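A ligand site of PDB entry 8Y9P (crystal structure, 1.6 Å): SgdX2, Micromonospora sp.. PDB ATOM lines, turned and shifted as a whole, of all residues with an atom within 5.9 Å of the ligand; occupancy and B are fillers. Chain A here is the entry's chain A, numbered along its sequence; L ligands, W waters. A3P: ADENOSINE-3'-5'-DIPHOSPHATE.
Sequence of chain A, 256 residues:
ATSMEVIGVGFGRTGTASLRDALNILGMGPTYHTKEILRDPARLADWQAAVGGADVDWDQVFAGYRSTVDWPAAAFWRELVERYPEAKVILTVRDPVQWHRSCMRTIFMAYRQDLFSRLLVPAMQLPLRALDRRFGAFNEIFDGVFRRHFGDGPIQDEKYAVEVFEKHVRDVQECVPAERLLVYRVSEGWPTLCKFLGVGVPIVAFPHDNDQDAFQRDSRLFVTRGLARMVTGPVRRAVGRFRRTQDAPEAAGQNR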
ATOM      1  N   PHE A  11     -13.372  -9.622 -22.372  1.00  0.00           N
ATOM      2  CA  PHE A  11     -13.274  -9.939 -23.789  1.00  0.00           C
ATOM      3  C   PHE A  11     -12.012 -10.782 -24.070  1.00  0.00           C
ATOM      4  O   PHE A  11     -11.058 -10.845 -23.274  1.00  0.00           O
ATOM      5  CB  PHE A  11     -13.187  -8.643 -24.599  1.00  0.00           C
ATOM      6  CG  PHE A  11     -14.473  -7.853 -24.688  1.00  0.00           C
ATOM      7  CD1 PHE A  11     -15.669  -8.349 -24.128  1.00  0.00           C
ATOM      8  CD2 PHE A  11     -14.489  -6.655 -25.376  1.00  0.00           C
ATOM      9  CE1 PHE A  11     -16.857  -7.620 -24.236  1.00  0.00           C
ATOM     10  CE2 PHE A  11     -15.681  -5.952 -25.494  1.00  0.00           C
ATOM     11  CZ  PHE A  11     -16.868  -6.436 -24.908  1.00  0.00           C
ATOM     12  N   GLY A  12     -11.975 -11.386 -25.251  1.00  0.00           N
ATOM     13  CA  GLY A  12     -10.727 -11.982 -25.710  1.00  0.00           C
ATOM     14  C   GLY A  12      -9.618 -10.957 -25.849  1.00  0.00           C
ATOM     15  O   GLY A  12      -9.865  -9.765 -26.004  1.00  0.00           O
ATOM     16  N   ARG A  13      -8.368 -11.439 -25.737  1.00  0.00           N
ATOM     17  CA  ARG A  13      -7.144 -10.588 -25.755  1.00  0.00           C
ATOM     18  C   ARG A  13      -7.063  -9.710 -24.517  1.00  0.00           C
ATOM     19  O   ARG A  13      -6.520  -8.617 -24.550  1.00  0.00           O
ATOM     20  CB  ARG A  13      -7.007  -9.719 -27.024  1.00  0.00           C
ATOM     21  CG  ARG A  13      -7.173 -10.467 -28.378  1.00  0.00           C
ATOM     22  CD  ARG A  13      -6.317 -11.746 -28.484  1.00  0.00           C
ATOM     23  NE  ARG A  13      -4.884 -11.469 -28.384  1.00  0.00           N
ATOM     24  CZ  ARG A  13      -3.953 -12.401 -28.556  1.00  0.00           C
ATOM     25  NH1 ARG A  13      -4.267 -13.619 -28.987  1.00  0.00           N
ATOM     26  NH2 ARG A  13      -2.679 -12.117 -28.308  1.00  0.00           N
ATOM     27  N   THR A  14      -7.526 -10.224 -23.383  1.00  0.00           N
ATOM     28  CA  THR A  14      -7.289  -9.570 -22.094  1.00  0.00           C
ATOM     29  C   THR A  14      -6.608 -10.508 -21.116  1.00  0.00           C
ATOM     30  O   THR A  14      -6.732 -10.338 -19.912  1.00  0.00           O
ATOM     31  CB  THR A  14      -8.609  -9.053 -21.494  1.00  0.00           C
ATOM     32  OG1 THR A  14      -9.504 -10.155 -21.250  1.00  0.00           O
ATOM     33  CG2 THR A  14      -9.317  -8.014 -22.405  1.00  0.00           C
ATOM     34  N   GLY A  15      -5.896 -11.517 -21.618  1.00  0.00           N
ATOM     35  CA  GLY A  15      -5.214 -12.477 -20.766  1.00  0.00           C
ATOM     36  C   GLY A  15      -6.058 -13.694 -20.412  1.00  0.00           C
ATOM     37  O   GLY A  15      -5.791 -14.329 -19.390  1.00  0.00           O
ATOM     38  N   THR A  16      -7.065 -14.014 -21.219  1.00  0.00           N
ATOM     39  CA  THR A  16      -7.985 -15.106 -20.865  1.00  0.00           C
ATOM     40  C   THR A  16      -7.307 -16.499 -20.899  1.00  0.00           C
ATOM     41  O   THR A  16      -7.695 -17.345 -20.095  1.00  0.00           O
ATOM     42  CB  THR A  16      -9.231 -15.118 -21.780  1.00  0.00           C
ATOM     43  OG1 THR A  16      -8.832 -15.398 -23.102  1.00  0.00           O
ATOM     44  CG2 THR A  16      -9.958 -13.769 -21.731  1.00  0.00           C
ATOM     45  N   ALA A  17      -6.337 -16.758 -21.797  1.00  0.00           N
ATOM     46  CA  ALA A  17      -5.666 -18.066 -21.748  1.00  0.00           C
ATOM     47  C   ALA A  17      -4.890 -18.216 -20.446  1.00  0.00           C
ATOM     48  O   ALA A  17      -4.914 -19.284 -19.807  1.00  0.00           O
ATOM     49  CB  ALA A  17      -4.756 -18.276 -22.970  1.00  0.00           C
ATOM     50  N   SER A  18      -4.212 -17.160 -20.011  1.00  0.00           N
ATOM     51  CA  SER A  18      -3.519 -17.238 -18.727  1.00  0.00           C
ATOM     52  C   SER A  18      -4.497 -17.402 -17.577  1.00  0.00           C
ATOM     53  O   SER A  18      -4.207 -18.161 -16.640  1.00  0.00           O
ATOM     54  CB  SER A  18      -2.633 -15.984 -18.504  1.00  0.00           C
ATOM     55  OG  SER A  18      -1.558 -15.986 -19.445  1.00  0.00           O
ATOM     56  N   HIS A  33     -13.028 -22.301 -22.656  1.00  0.00           N
ATOM     57  CA  HIS A  33     -12.264 -21.241 -23.322  1.00  0.00           C
ATOM     58  C   HIS A  33     -12.439 -21.512 -24.814  1.00  0.00           C
ATOM     59  O   HIS A  33     -12.815 -22.614 -25.183  1.00  0.00           O
ATOM     60  CB  HIS A  33     -10.767 -21.334 -22.916  1.00  0.00           C
ATOM     61  CG  HIS A  33      -9.860 -20.253 -23.465  1.00  0.00           C
ATOM     62  ND1 HIS A  33      -9.210 -20.387 -24.666  1.00  0.00           N
ATOM     63  CD2 HIS A  33      -9.467 -19.049 -22.964  1.00  0.00           C
ATOM     64  CE1 HIS A  33      -8.475 -19.310 -24.902  1.00  0.00           C
ATOM     65  NE2 HIS A  33      -8.619 -18.471 -23.884  1.00  0.00           N
ATOM     66  N   ASP A  70     -13.259 -16.100 -21.535  1.00  0.00           N
ATOM     67  CA  ASP A  70     -13.112 -15.757 -22.949  1.00  0.00           C
ATOM     68  C   ASP A  70     -14.466 -15.663 -23.648  1.00  0.00           C
ATOM     69  O   ASP A  70     -15.510 -16.079 -23.120  1.00  0.00           O
ATOM     70  CB  ASP A  70     -12.188 -16.805 -23.619  1.00  0.00           C
ATOM     71  CG  ASP A  70     -11.657 -16.431 -24.960  1.00  0.00           C
ATOM     72  OD1 ASP A  70     -11.725 -15.247 -25.378  1.00  0.00           O
ATOM     73  OD2 ASP A  70     -11.171 -17.399 -25.612  1.00  0.00           O
ATOM     74  N   ARG A  94      -7.848  -4.236 -19.654  1.00  0.00           N
ATOM     75  CA  ARG A  94      -6.611  -3.890 -20.340  1.00  0.00           C
ATOM     76  C   ARG A  94      -6.778  -2.469 -20.868  1.00  0.00           C
ATOM     77  O   ARG A  94      -7.915  -2.030 -21.057  1.00  0.00           O
ATOM     78  CB  ARG A  94      -6.440  -4.870 -21.503  1.00  0.00           C
ATOM     79  CG  ARG A  94      -5.223  -4.781 -22.143  1.00  0.00           C
ATOM     80  CD  ARG A  94      -5.209  -5.763 -23.279  1.00  0.00           C
ATOM     81  NE  ARG A  94      -3.876  -5.582 -23.799  1.00  0.00           N
ATOM     82  CZ  ARG A  94      -3.258  -6.375 -24.651  1.00  0.00           C
ATOM     83  NH1 ARG A  94      -3.855  -7.453 -25.144  1.00  0.00           N
ATOM     84  NH2 ARG A  94      -2.020  -6.081 -25.027  1.00  0.00           N
ATOM     85  N   GLN A  98      -4.627  -0.734 -26.528  1.00  0.00           N
ATOM     86  CA  GLN A  98      -3.766  -1.916 -26.674  1.00  0.00           C
ATOM     87  C   GLN A  98      -4.587  -3.148 -27.005  1.00  0.00           C
ATOM     88  O   GLN A  98      -4.159  -3.986 -27.824  1.00  0.00           O
ATOM     89  CB  GLN A  98      -2.992  -2.187 -25.372  1.00  0.00           C
ATOM     90  CG  GLN A  98      -1.930  -1.110 -25.111  1.00  0.00           C
ATOM     91  CD  GLN A  98      -0.968  -1.078 -26.224  1.00  0.00           C
ATOM     92  OE1 GLN A  98      -1.062  -0.242 -27.118  1.00  0.00           O
ATOM     93  NE2 GLN A  98      -0.030  -2.039 -26.215  1.00  0.00           N
ATOM     94  N   SER A 102      -4.228  -5.404 -30.412  1.00  0.00           N
ATOM     95  CA  SER A 102      -3.946  -6.839 -30.354  1.00  0.00           C
ATOM     96  C   SER A 102      -5.002  -7.627 -31.106  1.00  0.00           C
ATOM     97  O   SER A 102      -4.686  -8.564 -31.857  1.00  0.00           O
ATOM     98  CB  SER A 102      -3.874  -7.310 -28.906  1.00  0.00           C
ATOM     99  OG  SER A 102      -3.681  -8.723 -28.811  1.00  0.00           O
ATOM    100  N   ARG A 105      -4.611  -7.871 -34.868  1.00  0.00           N
ATOM    101  CA  ARG A 105      -3.551  -8.747 -35.336  1.00  0.00           C
ATOM    102  C   ARG A 105      -3.891 -10.214 -35.123  1.00  0.00           C
ATOM    103  O   ARG A 105      -3.151 -11.083 -35.585  1.00  0.00           O
ATOM    104  CB  ARG A 105      -2.231  -8.422 -34.626  1.00  0.00           C
ATOM    105  CG  ARG A 105      -1.649  -7.041 -34.949  1.00  0.00           C
ATOM    106  CD  ARG A 105      -0.258  -6.851 -34.338  1.00  0.00           C
ATOM    107  NE  ARG A 105      -0.307  -6.854 -32.875  1.00  0.00           N
ATOM    108  CZ  ARG A 105      -0.264  -5.752 -32.120  1.00  0.00           C
ATOM    109  NH1 ARG A 105      -0.110  -4.537 -32.650  1.00  0.00           N
ATOM    110  NH2 ARG A 105      -0.346  -5.868 -30.794  1.00  0.00           N
ATOM    111  N   VAL A 186      -4.326  -9.415 -15.703  1.00  0.00           N
ATOM    112  CA  VAL A 186      -3.491 -10.597 -15.479  1.00  0.00           C
ATOM    113  C   VAL A 186      -2.085 -10.213 -15.054  1.00  0.00           C
ATOM    114  O   VAL A 186      -1.412 -11.038 -14.429  1.00  0.00           O
ATOM    115  CB  VAL A 186      -3.439 -11.540 -16.716  1.00  0.00           C
ATOM    116  CG1 VAL A 186      -4.820 -12.265 -16.858  1.00  0.00           C
ATOM    117  CG2 VAL A 186      -3.031 -10.782 -17.997  1.00  0.00           C
ATOM    118  N   SER A 187      -1.620  -9.005 -15.377  1.00  0.00           N
ATOM    119  CA  SER A 187      -0.299  -8.639 -14.865  1.00  0.00           C
ATOM    120  C   SER A 187      -0.249  -8.559 -13.338  1.00  0.00           C
ATOM    121  O   SER A 187       0.851  -8.503 -12.783  1.00  0.00           O
ATOM    122  CB  SER A 187       0.173  -7.320 -15.499  1.00  0.00           C
ATOM    123  OG  SER A 187      -0.780  -6.291 -15.314  1.00  0.00           O
ATOM    124  N   PHE A 206       2.976 -17.651 -12.138  1.00  0.00           N
ATOM    125  CA  PHE A 206       1.694 -17.308 -12.736  1.00  0.00           C
ATOM    126  C   PHE A 206       1.776 -17.470 -14.257  1.00  0.00           C
ATOM    127  O   PHE A 206       2.795 -17.115 -14.860  1.00  0.00           O
ATOM    128  CB  PHE A 206       1.295 -15.874 -12.362  1.00  0.00           C
ATOM    129  CG  PHE A 206      -0.100 -15.502 -12.804  1.00  0.00           C
ATOM    130  CD1 PHE A 206      -1.219 -15.834 -12.035  1.00  0.00           C
ATOM    131  CD2 PHE A 206      -0.286 -14.818 -13.976  1.00  0.00           C
ATOM    132  CE1 PHE A 206      -2.481 -15.484 -12.450  1.00  0.00           C
ATOM    133  CE2 PHE A 206      -1.564 -14.479 -14.395  1.00  0.00           C
ATOM    134  CZ  PHE A 206      -2.656 -14.825 -13.642  1.00  0.00           C
ATOM    135  N   PRO A 207       0.730 -17.994 -14.904  1.00  0.00           N
ATOM    136  CA  PRO A 207       0.820 -18.269 -16.348  1.00  0.00           C
ATOM    137  C   PRO A 207       1.030 -17.008 -17.157  1.00  0.00           C
ATOM    138  O   PRO A 207       0.493 -15.942 -16.843  1.00  0.00           O
ATOM    139  CB  PRO A 207      -0.545 -18.888 -16.686  1.00  0.00           C
ATOM    140  CG  PRO A 207      -0.988 -19.493 -15.393  1.00  0.00           C
ATOM    141  CD  PRO A 207      -0.524 -18.502 -14.329  1.00  0.00           C
ATOM    142  N   HIS A 208       1.758 -17.166 -18.258  1.00  0.00           N
ATOM    143  CA  HIS A 208       1.922 -16.063 -19.221  1.00  0.00           C
ATOM    144  C   HIS A 208       1.797 -16.658 -20.614  1.00  0.00           C
ATOM    145  O   HIS A 208       2.792 -16.817 -21.317  1.00  0.00           O
ATOM    146  CB  HIS A 208       3.263 -15.326 -19.054  1.00  0.00           C
ATOM    147  CG  HIS A 208       3.282 -13.981 -19.700  1.00  0.00           C
ATOM    148  ND1 HIS A 208       2.672 -13.726 -20.919  1.00  0.00           N
ATOM    149  CD2 HIS A 208       3.831 -12.813 -19.313  1.00  0.00           C
ATOM    150  CE1 HIS A 208       2.839 -12.453 -21.236  1.00  0.00           C
ATOM    151  NE2 HIS A 208       3.536 -11.875 -20.281  1.00  0.00           N
ATOM    152  N   ASP A 209       0.574 -17.020 -20.985  1.00  0.00           N
ATOM    153  CA  ASP A 209       0.263 -17.580 -22.296  1.00  0.00           C
ATOM    154  C   ASP A 209       0.056 -16.412 -23.265  1.00  0.00           C
ATOM    155  O   ASP A 209      -0.914 -15.656 -23.135  1.00  0.00           O
ATOM    156  CB  ASP A 209      -0.993 -18.470 -22.196  1.00  0.00           C
ATOM    157  CG  ASP A 209      -1.278 -19.266 -23.495  1.00  0.00           C
ATOM    158  OD1 ASP A 209      -0.894 -18.812 -24.599  1.00  0.00           O
ATOM    159  OD2 ASP A 209      -1.850 -20.375 -23.405  1.00  0.00           O
ATOM    160  N   ASN A 210       0.973 -16.267 -24.232  1.00  0.00           N
ATOM    161  CA  ASN A 210       0.861 -15.142 -25.161  1.00  0.00           C
ATOM    162  C   ASN A 210      -0.267 -15.321 -26.165  1.00  0.00           C
ATOM    163  O   ASN A 210      -0.663 -14.343 -26.824  1.00  0.00           O
ATOM    164  CB  ASN A 210       2.193 -14.931 -25.893  1.00  0.00           C
ATOM    165  CG  ASN A 210       3.251 -14.311 -24.989  1.00  0.00           C
ATOM    166  OD1 ASN A 210       2.915 -13.550 -24.078  1.00  0.00           O
ATOM    167  ND2 ASN A 210       4.507 -14.632 -25.223  1.00  0.00           N
ATOM    168  N   ASP A 211      -0.803 -16.546 -26.274  1.00  0.00           N
ATOM    169  CA  ASP A 211      -1.982 -16.862 -27.105  1.00  0.00           C
ATOM    170  C   ASP A 211      -1.768 -16.441 -28.553  1.00  0.00           C
ATOM    171  O   ASP A 211      -2.634 -15.866 -29.207  1.00  0.00           O
ATOM    172  CB  ASP A 211      -3.265 -16.232 -26.518  1.00  0.00           C
ATOM    173  CG  ASP A 211      -4.523 -16.869 -27.061  1.00  0.00           C
ATOM    174  OD1 ASP A 211      -4.470 -18.056 -27.493  1.00  0.00           O
ATOM    175  OD2 ASP A 211      -5.565 -16.190 -27.066  1.00  0.00           O
ATOM    176  N   GLN A 212      -0.583 -16.758 -29.084  1.00  0.00           N
ATOM    177  CA  GLN A 212      -0.204 -16.303 -30.399  1.00  0.00           C
ATOM    178  C   GLN A 212      -0.140 -17.409 -31.440  1.00  0.00           C
ATOM    179  O   GLN A 212      -0.363 -17.151 -32.617  1.00  0.00           O
ATOM    180  CB  GLN A 212       1.158 -15.606 -30.342  1.00  0.00           C
ATOM    181  CG  GLN A 212       1.355 -14.591 -31.430  1.00  0.00           C
ATOM    182  CD  GLN A 212       0.152 -13.657 -31.593  1.00  0.00           C
ATOM    183  OE1 GLN A 212      -0.519 -13.670 -32.633  1.00  0.00           O
ATOM    184  NE2 GLN A 212      -0.108 -12.836 -30.564  1.00  0.00           N
HETATM  185  P1  A3P L   1      -1.036  -9.390 -26.501  1.00  0.00           P
HETATM  186  O1P A3P L   1      -2.576  -9.429 -26.774  1.00  0.00           O
HETATM  187  O2P A3P L   1      -0.142 -10.288 -27.448  1.00  0.00           O
HETATM  188  O3P A3P L   1      -0.446  -8.021 -26.456  1.00  0.00           O
HETATM  189  P2  A3P L   1      -5.805 -13.750 -24.472  1.00  0.00           P
HETATM  190  O4P A3P L   1      -5.216 -15.088 -23.820  1.00  0.00           O
HETATM  191  O5P A3P L   1      -5.775 -13.875 -25.949  1.00  0.00           O
HETATM  192  O6P A3P L   1      -7.135 -13.295 -23.906  1.00  0.00           O
HETATM  193  O5' A3P L   1      -4.767 -12.555 -24.106  1.00  0.00           O
HETATM  194  C5' A3P L   1      -3.442 -12.696 -24.593  1.00  0.00           C
HETATM  195  C4' A3P L   1      -2.711 -11.401 -24.189  1.00  0.00           C
HETATM  196  O4' A3P L   1      -2.517 -11.347 -22.752  1.00  0.00           O
HETATM  197  C3' A3P L   1      -1.295 -11.326 -24.787  1.00  0.00           C
HETATM  198  O3' A3P L   1      -0.882  -9.949 -24.987  1.00  0.00           O
HETATM  199  C2' A3P L   1      -0.434 -11.868 -23.653  1.00  0.00           C
HETATM  200  O2' A3P L   1       0.927 -11.463 -23.711  1.00  0.00           O
HETATM  201  C1' A3P L   1      -1.140 -11.205 -22.467  1.00  0.00           C
HETATM  202  N9  A3P L   1      -0.809 -11.835 -21.187  1.00  0.00           N
HETATM  203  C8  A3P L   1      -1.075 -13.152 -20.856  1.00  0.00           C
HETATM  204  N7  A3P L   1      -0.641 -13.487 -19.659  1.00  0.00           N
HETATM  205  C5  A3P L   1      -0.015 -12.350 -19.196  1.00  0.00           C
HETATM  206  C6  A3P L   1       0.601 -12.047 -17.970  1.00  0.00           C
HETATM  207  N6  A3P L   1       0.780 -12.949 -16.991  1.00  0.00           N
HETATM  208  N1  A3P L   1       1.105 -10.802 -17.801  1.00  0.00           N
HETATM  209  C2  A3P L   1       0.932  -9.904 -18.791  1.00  0.00           C
HETATM  210  N3  A3P L   1       0.318 -10.052 -19.962  1.00  0.00           N
HETATM  211  C4  A3P L   1      -0.145 -11.310 -20.114  1.00  0.00           C
HETATM  212  O   HOH W   1      -0.501  -7.382 -21.419  1.00  0.00           O
HETATM  213  O   HOH W   2       1.541 -11.900 -14.104  1.00  0.00           O
HETATM  214  O   HOH W   3      -1.373  -9.674 -30.337  1.00  0.00           O
HETATM  215  O   HOH W   4      -8.640 -14.255 -27.055  1.00  0.00           O
HETATM  216  O   HOH W   5      -3.799  -8.831 -21.674  1.00  0.00           O
HETATM  217  O   HOH W   6       3.185 -10.180 -16.054  1.00  0.00           O
HETATM  218  O   HOH W   7      -3.406 -15.096 -21.943  1.00  0.00           O
HETATM  219  O   HOH W   8       1.115  -7.805 -23.794  1.00  0.00           O
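Water W7 lies within hydrogen-bond range of O4P of the ligand (2.6 Å), O of Asp 209 (2.8 Å), N of Ser 18 (2.9 Å) and N of Ala 17 (3.4 Å). Water W5 bridges O4' of the ligand (3.0 Å) and N of Gly 15 (3.4 Å). Water W4 lies within hydrogen-bond range of O5P of the ligand and N of Arg 13. Water W2 bridges the backbone carbonyl oxygen (O) of Val 186 (3.1 Å) and a nitrogen (N6) of the ligand (3.2 Å). Water W3 lies within hydrogen-bond range of OG of Ser 102 (2.9 Å), O2P of the ligand (3.2 Å), NE2 of Gln 212 (3.4 Å) and NH2 of Arg 13 (3.4 Å).
The side-chain hydroxyl of Ser 102 sits at hydrogen-bond distance from an oxygen (O1P) of the ligand. O5P of the ligand sits close to OD2 of Asp 211 (2.6 Å). The side-chain hydroxyl (OG) of Ser 18 is in hydrogen-bond range of a nitrogen (N7) of the ligand (2.7 Å). O6P of the ligand lies within hydrogen-bond range of N of Thr 16 (2.8 Å). The side-chain hydroxyl (OG1) of Thr 16 sits at hydrogen-bond distance from an oxygen (O6P) of the ligand (2.8 Å). The backbone NH of Ala 17 lies within hydrogen-bond range of an oxygen (O4P) of the ligand (2.9 Å). The guanidinium group (NH1) of Arg 94 lies within salt-bridge range of an oxygen (O1P) of the ligand (2.9 Å). The backbone NH (N) of Arg 13 lies within hydrogen-bond range of an oxygen (O6P) of the ligand (2.9 Å). The guanidinium group of Arg 13 is in salt-bridge range of an oxygen (O1P) of the ligand, at 3.1 Å. The side-chain amide oxygen (OD1) of Asn 210 lies within hydrogen-bond range of an oxygen (O2') of the ligand (2.9 Å). N of Gly 15 is in hydrogen-bond range of O5' of the ligand, at 2.9 Å. O of Pro 207 lies within hydrogen-bond range of N6 of the ligand, 3.0 Å away. The backbone NH (N) of Thr 14 lies within hydrogen-bond range of an oxygen (O6P) of the ligand (3.1 Å).
The guanidinium group of Arg 13 lies within hydrogen-bond range of the side-chain hydroxyl of Ser 102 (3.0 Å). OD2 of Asp 211 is in salt-bridge range of NH1 of Arg 13. N of Asp 211 is in hydrogen-bond range of OD1 of Asp 209 (2.8 Å). O of Pro 207 sits at hydrogen-bond distance from OG of Ser 18, at 3.3 Å. OG1 of Thr 16 sits at hydrogen-bond distance from NE2 of His 33. The guanidinium group (NH2) of Arg 13 sits at hydrogen-bond distance from the backbone carbonyl oxygen (O) of Asn 210 (3.3 Å). OD1 of Asn 210 lies close to ND1 of His 208, at 3.2 Å. The side-chain hydroxyl (OG1) of Thr 14 lies within hydrogen-bond range of the backbone carbonyl oxygen (O) of Phe 11, 2.6 Å away.
Residues that only touch the ligand: His 208 (3.3 Å), Asp 209 (3.4 Å), Val 186 (3.6 Å), Phe 206 (3.7 Å), Ser 187 (3.9 Å) and Gly 12 (3.9 Å). Hydrophobic or aromatic side chains within 4 Å of the ligand: Ala 17, Val 186, Phe 206 and His 208. The nearest printed residue that does not touch the ligand is Gln 212 (4.03 Å).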
